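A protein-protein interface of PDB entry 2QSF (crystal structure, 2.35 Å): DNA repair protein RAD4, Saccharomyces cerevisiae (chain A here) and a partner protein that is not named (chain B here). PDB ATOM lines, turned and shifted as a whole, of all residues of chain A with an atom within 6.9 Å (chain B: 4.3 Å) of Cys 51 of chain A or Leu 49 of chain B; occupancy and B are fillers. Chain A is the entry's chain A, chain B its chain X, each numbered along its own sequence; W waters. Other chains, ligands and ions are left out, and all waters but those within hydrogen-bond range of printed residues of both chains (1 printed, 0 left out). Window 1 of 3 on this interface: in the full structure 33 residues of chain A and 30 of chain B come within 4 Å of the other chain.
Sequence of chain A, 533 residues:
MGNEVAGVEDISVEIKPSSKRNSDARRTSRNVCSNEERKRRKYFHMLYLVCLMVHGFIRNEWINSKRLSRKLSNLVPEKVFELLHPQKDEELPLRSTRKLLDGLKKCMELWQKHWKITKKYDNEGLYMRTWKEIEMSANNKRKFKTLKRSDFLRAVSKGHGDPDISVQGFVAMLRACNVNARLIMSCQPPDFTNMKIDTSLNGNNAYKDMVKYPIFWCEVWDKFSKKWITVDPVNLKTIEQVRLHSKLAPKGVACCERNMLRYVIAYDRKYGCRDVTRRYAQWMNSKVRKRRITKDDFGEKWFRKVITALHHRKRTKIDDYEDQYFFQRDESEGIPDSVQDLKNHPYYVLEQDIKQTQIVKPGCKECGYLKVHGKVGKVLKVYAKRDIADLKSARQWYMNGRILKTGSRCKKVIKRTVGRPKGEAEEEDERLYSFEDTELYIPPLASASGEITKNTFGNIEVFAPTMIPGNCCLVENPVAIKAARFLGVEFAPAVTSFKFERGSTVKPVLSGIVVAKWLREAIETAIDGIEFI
O of Leu 47 of chain A lies within hydrogen-bond range of SG of Cys 51 of chain A (3.4 Å). O of Ile 134 of chain A lies within hydrogen-bond range of OG of Ser 137 of chain A. OD1 of Asn 45 of chain B lies close to OE2 of Glu 47 of chain B (2.8 Å).
Among the printed residues, pairs that only touch across the chains: His 55 of chain A with Val 42 of chain B, Arg 129 of chain A with Ala 50 of chain B, His 55 of chain A with Pro 46 of chain B, Cys 51 of chain A with Val 42 of chain B, Val 54 of chain A with Val 42 of chain B, Ser 137 of chain A with Pro 51 of chain B, Leu 52 of chain A with Leu 49 of chain B, Cys 51 of chain A with Leu 49 of chain B, Tyr 48 of chain A with Leu 53 of chain B, Phe 144 of chain A with Ala 48 of chain B, Leu 126 of chain A with Pro 46 of chain B, Phe 144 of chain A with Glu 47 of chain B, Phe 44 of chain A with Leu 53 of chain B, Ser 137 of chain A with Ala 50 of chain B, Leu 126 of chain A with Glu 47 of chain B, Tyr 48 of chain A with Ala 50 of chain B and Phe 144 of chain A with Pro 51 of chain B.
Printed residues of chain B within 4 Å of Cys 51 of chain A: Val 42 (3.4 Å) and Leu 49 (3.7 Å). Printed residues of chain A within 4 Å of Leu 49 of chain B: Cys 51 (3.7 Å) and Leu 52 (3.6 Å). Of the printed residues of chain A, Pro 46 of chain B touches His 55 (3.4 Å) and Leu 126 (3.8 Å). Of the printed residues of chain B, Val 54 of chain A touches Val 42. Phe 57 of chain A touches none of the printed residues of chain B. The nearest residue of chain A that does not touch Leu 49 of chain B is Tyr 48 of chain A (4.3 Å).
Printed residues of chain A that touch a printed residue of chain B: Phe 44, Tyr 48, Cys 51, Leu 52, Val 54, His 55, Leu 126, Arg 129, Ser 137 and Phe 144. Printed residues of chain B that touch a printed residue of chain A: Val 42, Pro 46, Glu 47, Ala 48, Leu 49, Ala 50, Pro 51 and Leu 53. Hydrophobic or aromatic side chains of chain B within 4 Å of the printed part of chain A: Val 42, Pro 46, Ala 48, Leu 49, Ala 50, Pro 51 and Leu 53.
Water W1 lies within hydrogen-bond range of O of Glu 47 of chain B (3.0 Å), N of Ala 50 of chain B (3.0 Å) and OH of Tyr 48 of chain A (3.0 Å).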
ATOM      1  N   PHE A  44       1.617 -14.561  29.508  1.00  0.00           N
ATOM      2  CA  PHE A  44       2.074 -15.918  29.773  1.00  0.00           C
ATOM      3  C   PHE A  44       1.238 -16.878  28.949  1.00  0.00           C
ATOM      4  O   PHE A  44       1.746 -17.866  28.429  1.00  0.00           O
ATOM      5  CB  PHE A  44       1.929 -16.261  31.252  1.00  0.00           C
ATOM      6  CG  PHE A  44       2.834 -17.359  31.699  1.00  0.00           C
ATOM      7  CD1 PHE A  44       4.156 -17.084  32.054  1.00  0.00           C
ATOM      8  CD2 PHE A  44       2.389 -18.677  31.726  1.00  0.00           C
ATOM      9  CE1 PHE A  44       5.022 -18.106  32.428  1.00  0.00           C
ATOM     10  CE2 PHE A  44       3.249 -19.711  32.098  1.00  0.00           C
ATOM     11  CZ  PHE A  44       4.567 -19.424  32.449  1.00  0.00           C
ATOM     12  N   MET A  46      -0.026 -16.280  26.124  1.00  0.00           N
ATOM     13  CA  MET A  46       0.420 -16.161  24.747  1.00  0.00           C
ATOM     14  C   MET A  46       1.744 -16.873  24.535  1.00  0.00           C
ATOM     15  O   MET A  46       1.919 -17.607  23.560  1.00  0.00           O
ATOM     16  CB  MET A  46       0.534 -14.682  24.376  1.00  0.00           C
ATOM     17  CG  MET A  46      -0.808 -14.006  24.101  1.00  0.00           C
ATOM     18  SD  MET A  46      -0.691 -12.199  24.197  1.00  0.00           S
ATOM     19  CE  MET A  46       0.033 -11.807  22.628  1.00  0.00           C
ATOM     20  N   LEU A  47       2.666 -16.653  25.463  1.00  0.00           N
ATOM     21  CA  LEU A  47       3.986 -17.255  25.414  1.00  0.00           C
ATOM     22  C   LEU A  47       3.860 -18.781  25.391  1.00  0.00           C
ATOM     23  O   LEU A  47       4.489 -19.463  24.578  1.00  0.00           O
ATOM     24  CB  LEU A  47       4.771 -16.822  26.643  1.00  0.00           C
ATOM     25  CG  LEU A  47       6.281 -16.702  26.521  1.00  0.00           C
ATOM     26  CD1 LEU A  47       6.862 -17.007  27.875  1.00  0.00           C
ATOM     27  CD2 LEU A  47       6.821 -17.650  25.478  1.00  0.00           C
ATOM     28  N   TYR A  48       3.030 -19.301  26.290  1.00  0.00           N
ATOM     29  CA  TYR A  48       2.783 -20.740  26.420  1.00  0.00           C
ATOM     30  C   TYR A  48       2.129 -21.304  25.157  1.00  0.00           C
ATOM     31  O   TYR A  48       2.484 -22.376  24.685  1.00  0.00           O
ATOM     32  CB  TYR A  48       1.876 -20.957  27.629  1.00  0.00           C
ATOM     33  CG  TYR A  48       1.948 -22.305  28.287  1.00  0.00           C
ATOM     34  CD1 TYR A  48       2.579 -22.461  29.520  1.00  0.00           C
ATOM     35  CD2 TYR A  48       1.299 -23.406  27.735  1.00  0.00           C
ATOM     36  CE1 TYR A  48       2.550 -23.681  30.199  1.00  0.00           C
ATOM     37  CE2 TYR A  48       1.267 -24.630  28.397  1.00  0.00           C
ATOM     38  CZ  TYR A  48       1.888 -24.762  29.633  1.00  0.00           C
ATOM     39  OH  TYR A  48       1.819 -25.964  30.306  1.00  0.00           O
ATOM     40  N   LEU A  49       1.171 -20.564  24.609  1.00  0.00           N
ATOM     41  CA  LEU A  49       0.456 -20.960  23.393  1.00  0.00           C
ATOM     42  C   LEU A  49       1.385 -21.152  22.194  1.00  0.00           C
ATOM     43  O   LEU A  49       1.301 -22.160  21.496  1.00  0.00           O
ATOM     44  CB  LEU A  49      -0.564 -19.889  23.017  1.00  0.00           C
ATOM     45  CG  LEU A  49      -1.914 -20.305  22.437  1.00  0.00           C
ATOM     46  CD1 LEU A  49      -2.473 -19.141  21.646  1.00  0.00           C
ATOM     47  CD2 LEU A  49      -1.788 -21.505  21.566  1.00  0.00           C
ATOM     48  N   VAL A  50       2.237 -20.162  21.935  1.00  0.00           N
ATOM     49  CA  VAL A  50       3.157 -20.226  20.801  1.00  0.00           C
ATOM     50  C   VAL A  50       3.965 -21.498  20.901  1.00  0.00           C
ATOM     51  O   VAL A  50       3.999 -22.295  19.973  1.00  0.00           O
ATOM     52  CB  VAL A  50       4.146 -19.034  20.782  1.00  0.00           C
ATOM     53  CG1 VAL A  50       5.002 -19.103  19.540  1.00  0.00           C
ATOM     54  CG2 VAL A  50       3.394 -17.737  20.799  1.00  0.00           C
ATOM     55  N   CYS A  51       4.605 -21.682  22.048  1.00  0.00           N
ATOM     56  CA  CYS A  51       5.427 -22.858  22.307  1.00  0.00           C
ATOM     57  C   CYS A  51       4.702 -24.169  22.034  1.00  0.00           C
ATOM     58  O   CYS A  51       5.267 -25.077  21.421  1.00  0.00           O
ATOM     59  CB  CYS A  51       5.929 -22.816  23.741  1.00  0.00           C
ATOM     60  SG  CYS A  51       7.153 -21.526  24.011  1.00  0.00           S
ATOM     61  N   LEU A  52       3.450 -24.269  22.468  1.00  0.00           N
ATOM     62  CA  LEU A  52       2.675 -25.488  22.235  1.00  0.00           C
ATOM     63  C   LEU A  52       2.395 -25.707  20.759  1.00  0.00           C
ATOM     64  O   LEU A  52       2.344 -26.845  20.292  1.00  0.00           O
ATOM     65  CB  LEU A  52       1.339 -25.435  22.989  1.00  0.00           C
ATOM     66  CG  LEU A  52       1.382 -25.452  24.523  1.00  0.00           C
ATOM     67  CD1 LEU A  52      -0.009 -25.150  25.053  1.00  0.00           C
ATOM     68  CD2 LEU A  52       1.896 -26.813  25.034  1.00  0.00           C
ATOM     69  N   MET A  53       2.191 -24.613  20.026  1.00  0.00           N
ATOM     70  CA  MET A  53       1.895 -24.687  18.600  1.00  0.00           C
ATOM     71  C   MET A  53       3.180 -24.996  17.841  1.00  0.00           C
ATOM     72  O   MET A  53       3.160 -25.672  16.810  1.00  0.00           O
ATOM     73  CB  MET A  53       1.270 -23.374  18.124  1.00  0.00           C
ATOM     74  CG  MET A  53      -0.140 -23.134  18.664  1.00  0.00           C
ATOM     75  SD  MET A  53      -0.768 -21.498  18.248  1.00  0.00           S
ATOM     76  CE  MET A  53      -1.130 -21.738  16.470  1.00  0.00           C
ATOM     77  N   VAL A  54       4.297 -24.496  18.360  1.00  0.00           N
ATOM     78  CA  VAL A  54       5.582 -24.777  17.760  1.00  0.00           C
ATOM     79  C   VAL A  54       5.854 -26.249  18.033  1.00  0.00           C
ATOM     80  O   VAL A  54       6.321 -26.975  17.148  1.00  0.00           O
ATOM     81  CB  VAL A  54       6.690 -23.920  18.375  1.00  0.00           C
ATOM     82  CG1 VAL A  54       8.049 -24.496  18.006  1.00  0.00           C
ATOM     83  CG2 VAL A  54       6.575 -22.482  17.856  1.00  0.00           C
ATOM     84  N   HIS A  55       5.552 -26.702  19.251  1.00  0.00           N
ATOM     85  CA  HIS A  55       5.753 -28.112  19.574  1.00  0.00           C
ATOM     86  C   HIS A  55       4.987 -29.004  18.621  1.00  0.00           C
ATOM     87  O   HIS A  55       5.516 -29.989  18.132  1.00  0.00           O
ATOM     88  CB  HIS A  55       5.308 -28.452  20.994  1.00  0.00           C
ATOM     89  CG  HIS A  55       5.265 -29.927  21.263  1.00  0.00           C
ATOM     90  ND1 HIS A  55       4.102 -30.664  21.196  1.00  0.00           N
ATOM     91  CD2 HIS A  55       6.254 -30.814  21.526  1.00  0.00           C
ATOM     92  CE1 HIS A  55       4.376 -31.940  21.402  1.00  0.00           C
ATOM     93  NE2 HIS A  55       5.675 -32.059  21.605  1.00  0.00           N
ATOM     94  N   GLY A  56       3.727 -28.673  18.365  1.00  0.00           N
ATOM     95  CA  GLY A  56       2.942 -29.497  17.464  1.00  0.00           C
ATOM     96  C   GLY A  56       3.495 -29.494  16.053  1.00  0.00           C
ATOM     97  O   GLY A  56       3.344 -30.456  15.295  1.00  0.00           O
ATOM     98  N   PHE A  57       4.127 -28.388  15.691  1.00  0.00           N
ATOM     99  CA  PHE A  57       4.711 -28.248  14.372  1.00  0.00           C
ATOM    100  C   PHE A  57       5.887 -29.202  14.230  1.00  0.00           C
ATOM    101  O   PHE A  57       5.980 -29.942  13.254  1.00  0.00           O
ATOM    102  CB  PHE A  57       5.218 -26.822  14.160  1.00  0.00           C
ATOM    103  CG  PHE A  57       5.911 -26.626  12.843  1.00  0.00           C
ATOM    104  CD1 PHE A  57       5.189 -26.271  11.710  1.00  0.00           C
ATOM    105  CD2 PHE A  57       7.275 -26.859  12.723  1.00  0.00           C
ATOM    106  CE1 PHE A  57       5.813 -26.154  10.478  1.00  0.00           C
ATOM    107  CE2 PHE A  57       7.913 -26.747  11.494  1.00  0.00           C
ATOM    108  CZ  PHE A  57       7.177 -26.394  10.365  1.00  0.00           C
ATOM    109  N   LEU A 126      -0.239 -32.912  28.337  1.00  0.00           N
ATOM    110  CA  LEU A 126      -0.343 -31.552  27.822  1.00  0.00           C
ATOM    111  C   LEU A 126      -1.718 -30.941  28.090  1.00  0.00           C
ATOM    112  O   LEU A 126      -2.170 -30.050  27.373  1.00  0.00           O
ATOM    113  CB  LEU A 126      -0.015 -31.505  26.326  1.00  0.00           C
ATOM    114  CG  LEU A 126       1.448 -31.791  25.957  1.00  0.00           C
ATOM    115  CD1 LEU A 126       1.683 -31.379  24.515  1.00  0.00           C
ATOM    116  CD2 LEU A 126       2.387 -31.020  26.861  1.00  0.00           C
ATOM    117  N   ARG A 129      -2.989 -26.630  32.850  1.00  0.00           N
ATOM    118  CA  ARG A 129      -2.513 -26.517  34.217  1.00  0.00           C
ATOM    119  C   ARG A 129      -3.152 -25.259  34.775  1.00  0.00           C
ATOM    120  O   ARG A 129      -3.645 -24.435  34.014  1.00  0.00           O
ATOM    121  CB  ARG A 129      -0.988 -26.394  34.235  1.00  0.00           C
ATOM    122  CG  ARG A 129      -0.295 -27.600  33.601  1.00  0.00           C
ATOM    123  CD  ARG A 129       1.139 -27.312  33.215  1.00  0.00           C
ATOM    124  NE  ARG A 129       2.043 -27.271  34.360  1.00  0.00           N
ATOM    125  CZ  ARG A 129       2.327 -28.320  35.126  1.00  0.00           C
ATOM    126  NH1 ARG A 129       1.772 -29.499  34.872  1.00  0.00           N
ATOM    127  NH2 ARG A 129       3.177 -28.191  36.139  1.00  0.00           N
ATOM    128  N   ILE A 134       1.345 -23.675  37.916  1.00  0.00           N
ATOM    129  CA  ILE A 134       2.422 -23.061  37.146  1.00  0.00           C
ATOM    130  C   ILE A 134       3.335 -22.225  38.036  1.00  0.00           C
ATOM    131  O   ILE A 134       4.543 -22.176  37.820  1.00  0.00           O
ATOM    132  CB  ILE A 134       1.856 -22.194  36.006  1.00  0.00           C
ATOM    133  CG1 ILE A 134       1.084 -23.084  35.037  1.00  0.00           C
ATOM    134  CG2 ILE A 134       2.976 -21.482  35.266  1.00  0.00           C
ATOM    135  CD1 ILE A 134       0.530 -22.350  33.864  1.00  0.00           C
ATOM    136  N   SER A 137       5.466 -24.688  40.172  1.00  0.00           N
ATOM    137  CA  SER A 137       6.371 -25.572  39.447  1.00  0.00           C
ATOM    138  C   SER A 137       7.844 -25.297  39.747  1.00  0.00           C
ATOM    139  O   SER A 137       8.710 -26.099  39.406  1.00  0.00           O
ATOM    140  CB  SER A 137       6.107 -25.494  37.939  1.00  0.00           C
ATOM    141  OG  SER A 137       6.328 -24.188  37.443  1.00  0.00           O
ATOM    142  N   PHE A 144      12.961 -34.219  34.427  1.00  0.00           N
ATOM    143  CA  PHE A 144      12.377 -34.655  33.175  1.00  0.00           C
ATOM    144  C   PHE A 144      13.332 -35.571  32.426  1.00  0.00           C
ATOM    145  O   PHE A 144      14.538 -35.337  32.388  1.00  0.00           O
ATOM    146  CB  PHE A 144      12.026 -33.439  32.307  1.00  0.00           C
ATOM    147  CG  PHE A 144      11.064 -32.484  32.962  1.00  0.00           C
ATOM    148  CD1 PHE A 144       9.697 -32.704  32.906  1.00  0.00           C
ATOM    149  CD2 PHE A 144      11.538 -31.384  33.675  1.00  0.00           C
ATOM    150  CE1 PHE A 144       8.820 -31.856  33.547  1.00  0.00           C
ATOM    151  CE2 PHE A 144      10.667 -30.525  34.322  1.00  0.00           C
ATOM    152  CZ  PHE A 144       9.303 -30.762  34.260  1.00  0.00           C
ATOM    153  N   MET A 185      -4.076 -31.149  17.264  1.00  0.00           N
ATOM    154  CA  MET A 185      -3.648 -30.899  18.625  1.00  0.00           C
ATOM    155  C   MET A 185      -4.509 -29.805  19.235  1.00  0.00           C
ATOM    156  O   MET A 185      -4.600 -28.716  18.686  1.00  0.00           O
ATOM    157  CB  MET A 185      -2.188 -30.448  18.657  1.00  0.00           C
ATOM    158  CG  MET A 185      -1.723 -29.990  20.029  1.00  0.00           C
ATOM    159  SD  MET A 185      -0.043 -29.338  20.025  1.00  0.00           S
ATOM    160  CE  MET A 185       0.325 -29.254  21.720  1.00  0.00           C
ATOM    161  N   VAL A 306       1.313 -15.920  14.130  1.00  0.00           N
ATOM    162  CA  VAL A 306       1.799 -17.209  14.620  1.00  0.00           C
ATOM    163  C   VAL A 306       1.435 -18.356  13.688  1.00  0.00           C
ATOM    164  O   VAL A 306       2.274 -19.199  13.380  1.00  0.00           O
ATOM    165  CB  VAL A 306       1.247 -17.523  16.045  1.00  0.00           C
ATOM    166  CG1 VAL A 306       1.694 -18.910  16.487  1.00  0.00           C
ATOM    167  CG2 VAL A 306       1.745 -16.488  17.039  1.00  0.00           C
ATOM    168  N   VAL B  41      12.897 -28.570  25.198  1.00  0.00           N
ATOM    169  CA  VAL B  41      11.593 -28.585  25.833  1.00  0.00           C
ATOM    170  C   VAL B  41      10.426 -28.508  24.835  1.00  0.00           C
ATOM    171  O   VAL B  41       9.476 -29.292  24.928  1.00  0.00           O
ATOM    172  CB  VAL B  41      11.477 -27.439  26.851  1.00  0.00           C
ATOM    173  CG1 VAL B  41      10.007 -27.211  27.241  1.00  0.00           C
ATOM    174  CG2 VAL B  41      12.302 -27.780  28.086  1.00  0.00           C
ATOM    175  N   VAL B  42      10.490 -27.586  23.878  1.00  0.00           N
ATOM    176  CA  VAL B  42       9.405 -27.456  22.906  1.00  0.00           C
ATOM    177  C   VAL B  42       9.291 -28.605  21.917  1.00  0.00           C
ATOM    178  O   VAL B  42       8.212 -28.858  21.374  1.00  0.00           O
ATOM    179  CB  VAL B  42       9.523 -26.160  22.109  1.00  0.00           C
ATOM    180  CG1 VAL B  42       8.496 -26.138  21.003  1.00  0.00           C
ATOM    181  CG2 VAL B  42       9.299 -24.981  23.028  1.00  0.00           C
ATOM    182  N   ASN B  45      10.121 -32.365  25.210  1.00  0.00           N
ATOM    183  CA  ASN B  45       9.559 -32.389  26.550  1.00  0.00           C
ATOM    184  C   ASN B  45       8.686 -31.192  26.873  1.00  0.00           C
ATOM    185  O   ASN B  45       8.962 -30.448  27.814  1.00  0.00           O
ATOM    186  CB  ASN B  45      10.692 -32.505  27.563  1.00  0.00           C
ATOM    187  CG  ASN B  45      11.431 -33.829  27.452  1.00  0.00           C
ATOM    188  OD1 ASN B  45      10.991 -34.843  27.989  1.00  0.00           O
ATOM    189  ND2 ASN B  45      12.546 -33.828  26.733  1.00  0.00           N
ATOM    190  N   PRO B  46       7.595 -31.010  26.114  1.00  0.00           N
ATOM    191  CA  PRO B  46       6.676 -29.889  26.328  1.00  0.00           C
ATOM    192  C   PRO B  46       6.053 -29.852  27.720  1.00  0.00           C
ATOM    193  O   PRO B  46       5.604 -28.795  28.180  1.00  0.00           O
ATOM    194  CB  PRO B  46       5.649 -30.060  25.210  1.00  0.00           C
ATOM    195  CG  PRO B  46       5.668 -31.537  24.935  1.00  0.00           C
ATOM    196  CD  PRO B  46       7.126 -31.882  25.020  1.00  0.00           C
ATOM    197  N   GLU B  47       6.037 -30.993  28.403  1.00  0.00           N
ATOM    198  CA  GLU B  47       5.487 -31.047  29.754  1.00  0.00           C
ATOM    199  C   GLU B  47       6.354 -30.208  30.695  1.00  0.00           C
ATOM    200  O   GLU B  47       5.972 -29.935  31.837  1.00  0.00           O
ATOM    201  CB  GLU B  47       5.403 -32.498  30.250  1.00  0.00           C
ATOM    202  CG  GLU B  47       6.744 -33.225  30.427  1.00  0.00           C
ATOM    203  CD  GLU B  47       7.387 -33.714  29.116  1.00  0.00           C
ATOM    204  OE1 GLU B  47       6.759 -33.613  28.034  1.00  0.00           O
ATOM    205  OE2 GLU B  47       8.533 -34.212  29.176  1.00  0.00           O
ATOM    206  N   ALA B  48       7.519 -29.781  30.214  1.00  0.00           N
ATOM    207  CA  ALA B  48       8.408 -28.949  31.028  1.00  0.00           C
ATOM    208  C   ALA B  48       8.242 -27.454  30.711  1.00  0.00           C
ATOM    209  O   ALA B  48       8.944 -26.616  31.285  1.00  0.00           O
ATOM    210  CB  ALA B  48       9.878 -29.374  30.826  1.00  0.00           C
ATOM    211  N   LEU B  49       7.315 -27.122  29.808  1.00  0.00           N
ATOM    212  CA  LEU B  49       7.075 -25.727  29.447  1.00  0.00           C
ATOM    213  C   LEU B  49       6.780 -24.817  30.630  1.00  0.00           C
ATOM    214  O   LEU B  49       7.328 -23.716  30.718  1.00  0.00           O
ATOM    215  CB  LEU B  49       5.938 -25.611  28.426  1.00  0.00           C
ATOM    216  CG  LEU B  49       6.381 -25.841  26.977  1.00  0.00           C
ATOM    217  CD1 LEU B  49       5.198 -25.876  26.051  1.00  0.00           C
ATOM    218  CD2 LEU B  49       7.345 -24.741  26.583  1.00  0.00           C
ATOM    219  N   ALA B  50       5.927 -25.266  31.546  1.00  0.00           N
ATOM    220  CA  ALA B  50       5.571 -24.443  32.705  1.00  0.00           C
ATOM    221  C   ALA B  50       6.781 -24.009  33.532  1.00  0.00           C
ATOM    222  O   ALA B  50       7.033 -22.813  33.686  1.00  0.00           O
ATOM    223  CB  ALA B  50       4.566 -25.179  33.584  1.00  0.00           C
ATOM    224  N   PRO B  51       7.548 -24.964  34.087  1.00  0.00           N
ATOM    225  CA  PRO B  51       8.697 -24.501  34.869  1.00  0.00           C
ATOM    226  C   PRO B  51       9.738 -23.759  34.031  1.00  0.00           C
ATOM    227  O   PRO B  51      10.398 -22.844  34.525  1.00  0.00           O
ATOM    228  CB  PRO B  51       9.249 -25.793  35.464  1.00  0.00           C
ATOM    229  CG  PRO B  51       8.909 -26.813  34.424  1.00  0.00           C
ATOM    230  CD  PRO B  51       7.481 -26.435  34.089  1.00  0.00           C
ATOM    231  N   LEU B  52       9.882 -24.137  32.765  1.00  0.00           N
ATOM    232  CA  LEU B  52      10.876 -23.492  31.912  1.00  0.00           C
ATOM    233  C   LEU B  52      10.534 -22.042  31.574  1.00  0.00           C
ATOM    234  O   LEU B  52      11.396 -21.167  31.670  1.00  0.00           O
ATOM    235  CB  LEU B  52      11.085 -24.305  30.635  1.00  0.00           C
ATOM    236  CG  LEU B  52      12.288 -23.971  29.733  1.00  0.00           C
ATOM    237  CD1 LEU B  52      11.920 -22.853  28.799  1.00  0.00           C
ATOM    238  CD2 LEU B  52      13.516 -23.601  30.571  1.00  0.00           C
ATOM    239  N   LEU B  53       9.281 -21.792  31.198  1.00  0.00           N
ATOM    240  CA  LEU B  53       8.832 -20.442  30.863  1.00  0.00           C
ATOM    241  C   LEU B  53       8.733 -19.523  32.081  1.00  0.00           C
ATOM    242  O   LEU B  53       8.838 -18.307  31.947  1.00  0.00           O
ATOM    243  CB  LEU B  53       7.482 -20.489  30.143  1.00  0.00           C
ATOM    244  CG  LEU B  53       7.446 -21.228  28.797  1.00  0.00           C
ATOM    245  CD1 LEU B  53       6.062 -21.088  28.153  1.00  0.00           C
ATOM    246  CD2 LEU B  53       8.527 -20.658  27.878  1.00  0.00           C
ATOM    247  N   PHE B  74      10.249 -15.016  17.212  1.00  0.00           N
ATOM    248  CA  PHE B  74      10.481 -15.996  18.271  1.00  0.00           C
ATOM    249  C   PHE B  74      10.218 -17.399  17.723  1.00  0.00           C
ATOM    250  O   PHE B  74      10.931 -18.348  18.039  1.00  0.00           O
ATOM    251  CB  PHE B  74       9.558 -15.686  19.449  1.00  0.00           C
ATOM    252  CG  PHE B  74       9.682 -16.642  20.595  1.00  0.00           C
ATOM    253  CD1 PHE B  74       8.756 -17.666  20.767  1.00  0.00           C
ATOM    254  CD2 PHE B  74      10.715 -16.511  21.513  1.00  0.00           C
ATOM    255  CE1 PHE B  74       8.857 -18.541  21.832  1.00  0.00           C
ATOM    256  CE2 PHE B  74      10.823 -17.387  22.585  1.00  0.00           C
ATOM    257  CZ  PHE B  74       9.898 -18.398  22.746  1.00  0.00           C
HETATM  258  O   HOH W   1       4.135 -27.644  31.281  1.00  0.00           O
